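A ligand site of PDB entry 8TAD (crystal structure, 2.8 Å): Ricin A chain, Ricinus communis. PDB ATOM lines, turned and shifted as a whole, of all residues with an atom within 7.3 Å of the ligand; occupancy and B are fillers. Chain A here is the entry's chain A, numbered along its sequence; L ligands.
The guanidinium group of Arg 232 lies within salt-bridge range of an oxygen (O2) of the ligand (3.0 Å).
An oxygen (O1) of the ligand lies within salt-bridge range of the guanidinium group (NE) of Arg 231 (3.8 Å).
The side-chain amide nitrogen (NE2) of Gln 230 lies close to the side-chain hydroxyl (OG1) of Thr 203, at 3.3 Å.
O of Phe 237 is in hydrogen-bond range of N of Leu 229 (3.2 Å).
The side-chain hydroxyl of Ser 200 is in hydrogen-bond range of the side-chain hydroxyl of Tyr 180, 2.7 Å away.
Residues that only touch the ligand: Tyr 180 (3.6 Å), Leu 204 (3.6 Å), Leu 229 (3.7 Å), Gln 230 (3.5 Å), Phe 237 (3.6 Å), Ile 244 (3.9 Å) and Ile 248 (3.7 Å).
Hydrophobic or aromatic side chains that line the ligand: Tyr 180, Leu 204, Leu 229, Phe 237, Ile 244 and Ile 248.
Of the 20 residues printed, 9 come within 4 Å of the ligand.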
ATOM      1  N   PHE A 178     -17.639 -19.882  -1.013  1.00  0.00           N
ATOM      2  CA  PHE A 178     -17.413 -19.296   0.300  1.00  0.00           C
ATOM      3  C   PHE A 178     -15.970 -19.533   0.721  1.00  0.00           C
ATOM      4  O   PHE A 178     -15.497 -20.679   0.692  1.00  0.00           O
ATOM      5  CB  PHE A 178     -18.358 -19.887   1.350  1.00  0.00           C
ATOM      6  CG  PHE A 178     -19.816 -19.678   1.035  1.00  0.00           C
ATOM      7  CD1 PHE A 178     -20.460 -18.512   1.399  1.00  0.00           C
ATOM      8  CD2 PHE A 178     -20.544 -20.671   0.400  1.00  0.00           C
ATOM      9  CE1 PHE A 178     -21.802 -18.325   1.112  1.00  0.00           C
ATOM     10  CE2 PHE A 178     -21.888 -20.494   0.113  1.00  0.00           C
ATOM     11  CZ  PHE A 178     -22.514 -19.312   0.477  1.00  0.00           C
ATOM     12  N   TYR A 180     -15.290 -19.140   3.791  1.00  0.00           N
ATOM     13  CA  TYR A 180     -15.526 -19.801   5.069  1.00  0.00           C
ATOM     14  C   TYR A 180     -15.547 -21.316   4.921  1.00  0.00           C
ATOM     15  O   TYR A 180     -14.959 -22.048   5.728  1.00  0.00           O
ATOM     16  CB  TYR A 180     -16.840 -19.319   5.677  1.00  0.00           C
ATOM     17  CG  TYR A 180     -17.195 -20.024   6.969  1.00  0.00           C
ATOM     18  CD1 TYR A 180     -16.297 -20.092   8.017  1.00  0.00           C
ATOM     19  CD2 TYR A 180     -18.438 -20.634   7.129  1.00  0.00           C
ATOM     20  CE1 TYR A 180     -16.623 -20.741   9.199  1.00  0.00           C
ATOM     21  CE2 TYR A 180     -18.768 -21.291   8.296  1.00  0.00           C
ATOM     22  CZ  TYR A 180     -17.850 -21.332   9.331  1.00  0.00           C
ATOM     23  OH  TYR A 180     -18.178 -21.979  10.499  1.00  0.00           O
ATOM     24  N   ILE A 181     -16.216 -21.816   3.878  1.00  0.00           N
ATOM     25  CA  ILE A 181     -16.300 -23.257   3.673  1.00  0.00           C
ATOM     26  C   ILE A 181     -14.944 -23.809   3.231  1.00  0.00           C
ATOM     27  O   ILE A 181     -14.542 -24.908   3.638  1.00  0.00           O
ATOM     28  CB  ILE A 181     -17.409 -23.596   2.666  1.00  0.00           C
ATOM     29  CG1 ILE A 181     -18.762 -23.696   3.389  1.00  0.00           C
ATOM     30  CG2 ILE A 181     -17.125 -24.901   1.933  1.00  0.00           C
ATOM     31  CD1 ILE A 181     -19.955 -23.393   2.508  1.00  0.00           C
ATOM     32  N   ASP A 198     -20.946 -28.609  10.250  1.00  0.00           N
ATOM     33  CA  ASP A 198     -21.707 -28.050  11.357  1.00  0.00           C
ATOM     34  C   ASP A 198     -22.767 -27.091  10.833  1.00  0.00           C
ATOM     35  O   ASP A 198     -22.662 -26.599   9.710  1.00  0.00           O
ATOM     36  CB  ASP A 198     -20.747 -27.337  12.326  1.00  0.00           C
ATOM     37  CG  ASP A 198     -19.889 -26.304  11.635  1.00  0.00           C
ATOM     38  OD1 ASP A 198     -20.427 -25.253  11.229  1.00  0.00           O
ATOM     39  OD2 ASP A 198     -18.670 -26.530  11.499  1.00  0.00           O
ATOM     40  N   PRO A 199     -23.826 -26.808  11.633  1.00  0.00           N
ATOM     41  CA  PRO A 199     -24.965 -26.027  11.116  1.00  0.00           C
ATOM     42  C   PRO A 199     -24.607 -24.676  10.501  1.00  0.00           C
ATOM     43  O   PRO A 199     -25.427 -24.101   9.782  1.00  0.00           O
ATOM     44  CB  PRO A 199     -25.861 -25.820  12.356  1.00  0.00           C
ATOM     45  CG  PRO A 199     -25.384 -26.762  13.378  1.00  0.00           C
ATOM     46  CD  PRO A 199     -24.027 -27.261  13.021  1.00  0.00           C
ATOM     47  N   SER A 200     -23.406 -24.160  10.762  1.00  0.00           N
ATOM     48  CA  SER A 200     -22.992 -22.906  10.137  1.00  0.00           C
ATOM     49  C   SER A 200     -22.647 -23.083   8.668  1.00  0.00           C
ATOM     50  O   SER A 200     -22.616 -22.102   7.924  1.00  0.00           O
ATOM     51  CB  SER A 200     -21.802 -22.301  10.876  1.00  0.00           C
ATOM     52  OG  SER A 200     -20.613 -23.036  10.614  1.00  0.00           O
ATOM     53  N   VAL A 201     -22.395 -24.317   8.235  1.00  0.00           N
ATOM     54  CA  VAL A 201     -22.025 -24.581   6.846  1.00  0.00           C
ATOM     55  C   VAL A 201     -23.245 -24.917   5.993  1.00  0.00           C
ATOM     56  O   VAL A 201     -23.415 -24.368   4.906  1.00  0.00           O
ATOM     57  CB  VAL A 201     -20.982 -25.713   6.777  1.00  0.00           C
ATOM     58  CG1 VAL A 201     -20.805 -26.171   5.332  1.00  0.00           C
ATOM     59  CG2 VAL A 201     -19.667 -25.227   7.345  1.00  0.00           C
ATOM     60  N   THR A 203     -26.204 -23.948   6.584  1.00  0.00           N
ATOM     61  CA  THR A 203     -26.944 -22.691   6.496  1.00  0.00           C
ATOM     62  C   THR A 203     -26.390 -21.788   5.403  1.00  0.00           C
ATOM     63  O   THR A 203     -27.163 -21.161   4.665  1.00  0.00           O
ATOM     64  CB  THR A 203     -26.941 -21.959   7.850  1.00  0.00           C
ATOM     65  OG1 THR A 203     -27.556 -22.796   8.850  1.00  0.00           O
ATOM     66  CG2 THR A 203     -27.732 -20.668   7.757  1.00  0.00           C
ATOM     67  N   LEU A 204     -25.062 -21.710   5.259  1.00  0.00           N
ATOM     68  CA  LEU A 204     -24.488 -20.886   4.190  1.00  0.00           C
ATOM     69  C   LEU A 204     -24.808 -21.463   2.816  1.00  0.00           C
ATOM     70  O   LEU A 204     -25.157 -20.719   1.900  1.00  0.00           O
ATOM     71  CB  LEU A 204     -22.977 -20.762   4.349  1.00  0.00           C
ATOM     72  CG  LEU A 204     -22.427 -19.620   5.199  1.00  0.00           C
ATOM     73  CD1 LEU A 204     -20.922 -19.578   5.069  1.00  0.00           C
ATOM     74  CD2 LEU A 204     -23.045 -18.288   4.779  1.00  0.00           C
ATOM     75  N   LEU A 229     -28.260 -16.195   9.477  1.00  0.00           N
ATOM     76  CA  LEU A 229     -27.259 -17.247   9.444  1.00  0.00           C
ATOM     77  C   LEU A 229     -27.253 -17.996  10.766  1.00  0.00           C
ATOM     78  O   LEU A 229     -28.018 -17.687  11.691  1.00  0.00           O
ATOM     79  CB  LEU A 229     -25.875 -16.668   9.129  1.00  0.00           C
ATOM     80  CG  LEU A 229     -25.445 -16.361   7.693  1.00  0.00           C
ATOM     81  CD1 LEU A 229     -26.587 -15.874   6.809  1.00  0.00           C
ATOM     82  CD2 LEU A 229     -24.307 -15.355   7.680  1.00  0.00           C
ATOM     83  N   GLN A 230     -26.390 -18.997  10.874  1.00  0.00           N
ATOM     84  CA  GLN A 230     -26.278 -19.812  12.070  1.00  0.00           C
ATOM     85  C   GLN A 230     -24.831 -19.847  12.537  1.00  0.00           C
ATOM     86  O   GLN A 230     -23.924 -20.060  11.739  1.00  0.00           O
ATOM     87  CB  GLN A 230     -26.769 -21.248  11.828  1.00  0.00           C
ATOM     88  CG  GLN A 230     -28.261 -21.369  11.581  1.00  0.00           C
ATOM     89  CD  GLN A 230     -28.780 -22.761  11.885  1.00  0.00           C
ATOM     90  OE1 GLN A 230     -28.198 -23.491  12.701  1.00  0.00           O
ATOM     91  NE2 GLN A 230     -29.863 -23.153  11.233  1.00  0.00           N
ATOM     92  N   ARG A 231     -24.632 -19.637  13.841  1.00  0.00           N
ATOM     93  CA  ARG A 231     -23.334 -19.927  14.434  1.00  0.00           C
ATOM     94  C   ARG A 231     -23.144 -21.445  14.500  1.00  0.00           C
ATOM     95  O   ARG A 231     -24.080 -22.228  14.357  1.00  0.00           O
ATOM     96  CB  ARG A 231     -23.226 -19.298  15.829  1.00  0.00           C
ATOM     97  CG  ARG A 231     -23.484 -17.801  15.838  1.00  0.00           C
ATOM     98  CD  ARG A 231     -23.253 -17.160  17.201  1.00  0.00           C
ATOM     99  NE  ARG A 231     -22.543 -15.898  17.083  1.00  0.00           N
ATOM    100  CZ  ARG A 231     -21.875 -15.309  18.066  1.00  0.00           C
ATOM    101  NH1 ARG A 231     -21.841 -15.826  19.286  1.00  0.00           N
ATOM    102  NH2 ARG A 231     -21.244 -14.161  17.835  1.00  0.00           N
ATOM    103  N   ARG A 232     -21.889 -21.851  14.703  1.00  0.00           N
ATOM    104  CA  ARG A 232     -21.555 -23.266  14.618  1.00  0.00           C
ATOM    105  C   ARG A 232     -22.244 -24.111  15.689  1.00  0.00           C
ATOM    106  O   ARG A 232     -22.371 -25.327  15.517  1.00  0.00           O
ATOM    107  CB  ARG A 232     -20.035 -23.457  14.700  1.00  0.00           C
ATOM    108  CG  ARG A 232     -19.270 -22.569  13.734  1.00  0.00           C
ATOM    109  CD  ARG A 232     -17.803 -22.961  13.681  1.00  0.00           C
ATOM    110  NE  ARG A 232     -17.042 -22.343  14.759  1.00  0.00           N
ATOM    111  CZ  ARG A 232     -16.300 -23.017  15.631  1.00  0.00           C
ATOM    112  NH1 ARG A 232     -16.201 -24.334  15.581  1.00  0.00           N
ATOM    113  NH2 ARG A 232     -15.646 -22.348  16.582  1.00  0.00           N
ATOM    114  N   ASN A 233     -22.706 -23.492  16.781  1.00  0.00           N
ATOM    115  CA  ASN A 233     -23.449 -24.206  17.810  1.00  0.00           C
ATOM    116  C   ASN A 233     -24.951 -24.278  17.513  1.00  0.00           C
ATOM    117  O   ASN A 233     -25.719 -24.728  18.370  1.00  0.00           O
ATOM    118  CB  ASN A 233     -23.210 -23.567  19.178  1.00  0.00           C
ATOM    119  CG  ASN A 233     -23.739 -22.144  19.277  1.00  0.00           C
ATOM    120  OD1 ASN A 233     -24.281 -21.596  18.319  1.00  0.00           O
ATOM    121  ND2 ASN A 233     -23.578 -21.538  20.448  1.00  0.00           N
ATOM    122  N   SER A 235     -27.040 -21.761  17.219  1.00  0.00           N
ATOM    123  CA  SER A 235     -27.697 -20.504  17.538  1.00  0.00           C
ATOM    124  C   SER A 235     -27.621 -19.551  16.349  1.00  0.00           C
ATOM    125  O   SER A 235     -26.642 -19.548  15.585  1.00  0.00           O
ATOM    126  CB  SER A 235     -27.064 -19.859  18.768  1.00  0.00           C
ATOM    127  OG  SER A 235     -25.704 -19.541  18.537  1.00  0.00           O
ATOM    128  N   PHE A 237     -28.292 -15.725  14.197  1.00  0.00           N
ATOM    129  CA  PHE A 237     -28.184 -14.273  14.228  1.00  0.00           C
ATOM    130  C   PHE A 237     -28.653 -13.754  12.873  1.00  0.00           C
ATOM    131  O   PHE A 237     -29.146 -14.516  12.030  1.00  0.00           O
ATOM    132  CB  PHE A 237     -26.754 -13.836  14.586  1.00  0.00           C
ATOM    133  CG  PHE A 237     -25.706 -14.274  13.602  1.00  0.00           C
ATOM    134  CD1 PHE A 237     -25.505 -13.591  12.408  1.00  0.00           C
ATOM    135  CD2 PHE A 237     -24.918 -15.376  13.877  1.00  0.00           C
ATOM    136  CE1 PHE A 237     -24.535 -14.008  11.513  1.00  0.00           C
ATOM    137  CE2 PHE A 237     -23.948 -15.793  12.982  1.00  0.00           C
ATOM    138  CZ  PHE A 237     -23.753 -15.109  11.796  1.00  0.00           C
ATOM    139  N   VAL A 239     -27.537 -10.724   9.761  1.00  0.00           N
ATOM    140  CA  VAL A 239     -26.681  -9.665   9.231  1.00  0.00           C
ATOM    141  C   VAL A 239     -27.534  -8.756   8.365  1.00  0.00           C
ATOM    142  O   VAL A 239     -28.564  -9.161   7.806  1.00  0.00           O
ATOM    143  CB  VAL A 239     -25.484 -10.235   8.451  1.00  0.00           C
ATOM    144  CG1 VAL A 239     -24.874 -11.412   9.193  1.00  0.00           C
ATOM    145  CG2 VAL A 239     -25.880 -10.622   7.037  1.00  0.00           C
ATOM    146  N   ILE A 244     -19.949  -7.389   6.494  1.00  0.00           N
ATOM    147  CA  ILE A 244     -19.651  -8.511   7.382  1.00  0.00           C
ATOM    148  C   ILE A 244     -19.482  -9.814   6.611  1.00  0.00           C
ATOM    149  O   ILE A 244     -18.873 -10.761   7.138  1.00  0.00           O
ATOM    150  CB  ILE A 244     -20.745  -8.641   8.462  1.00  0.00           C
ATOM    151  CG1 ILE A 244     -20.303  -9.594   9.572  1.00  0.00           C
ATOM    152  CG2 ILE A 244     -22.049  -9.114   7.837  1.00  0.00           C
ATOM    153  CD1 ILE A 244     -18.931  -9.287  10.126  1.00  0.00           C
ATOM    154  N   LEU A 245     -19.977  -9.893   5.382  1.00  0.00           N
ATOM    155  CA  LEU A 245     -19.884 -11.101   4.581  1.00  0.00           C
ATOM    156  C   LEU A 245     -18.784 -11.047   3.525  1.00  0.00           C
ATOM    157  O   LEU A 245     -18.611 -12.022   2.789  1.00  0.00           O
ATOM    158  CB  LEU A 245     -21.234 -11.369   3.900  1.00  0.00           C
ATOM    159  CG  LEU A 245     -22.454 -11.326   4.815  1.00  0.00           C
ATOM    160  CD1 LEU A 245     -23.733 -11.350   4.001  1.00  0.00           C
ATOM    161  CD2 LEU A 245     -22.413 -12.476   5.810  1.00  0.00           C
ATOM    162  N   ILE A 248     -16.481 -13.774   3.714  1.00  0.00           N
ATOM    163  CA  ILE A 248     -17.262 -14.985   3.924  1.00  0.00           C
ATOM    164  C   ILE A 248     -17.744 -15.599   2.618  1.00  0.00           C
ATOM    165  O   ILE A 248     -17.766 -16.824   2.478  1.00  0.00           O
ATOM    166  CB  ILE A 248     -18.446 -14.696   4.881  1.00  0.00           C
ATOM    167  CG1 ILE A 248     -17.916 -14.321   6.273  1.00  0.00           C
ATOM    168  CG2 ILE A 248     -19.379 -15.897   4.971  1.00  0.00           C
ATOM    169  CD1 ILE A 248     -17.021 -15.370   6.880  1.00  0.00           C
HETATM  170  C1  LIG L   1     -19.429 -19.060  15.531  1.00  0.00           C
HETATM  171  C2  LIG L   1     -20.260 -15.697  11.216  1.00  0.00           C
HETATM  172  C3  LIG L   1     -20.842 -15.037   8.958  1.00  0.00           C
HETATM  173  C4  LIG L   1     -20.334 -13.355  10.613  1.00  0.00           C
HETATM  174  C5  LIG L   1     -22.269 -17.883   9.625  1.00  0.00           C
HETATM  175  C6  LIG L   1     -20.798 -17.513   9.526  1.00  0.00           C
HETATM  176  C7  LIG L   1     -20.346 -17.679   8.077  1.00  0.00           C
HETATM  177  C8  LIG L   1     -20.021 -18.471  10.350  1.00  0.00           C
HETATM  178  C9  LIG L   1     -19.920 -18.087  11.815  1.00  0.00           C
HETATM  179  C10 LIG L   1     -20.046 -16.736  12.208  1.00  0.00           C
HETATM  180  C11 LIG L   1     -19.653 -18.376  14.172  1.00  0.00           C
HETATM  181  C12 LIG L   1     -19.703 -18.991  12.910  1.00  0.00           C
HETATM  182  C13 LIG L   1     -20.631 -16.040   9.919  1.00  0.00           C
HETATM  183  C14 LIG L   1     -20.698 -13.699   9.308  1.00  0.00           C
HETATM  184  C15 LIG L   1     -20.114 -14.350  11.567  1.00  0.00           C
HETATM  185  O1  LIG L   1     -20.120 -18.725  16.524  1.00  0.00           O
HETATM  186  O2  LIG L   1     -18.548 -19.962  15.643  1.00  0.00           O
HETATM  187  S1  LIG L   1     -19.878 -16.713  13.899  1.00  0.00           S
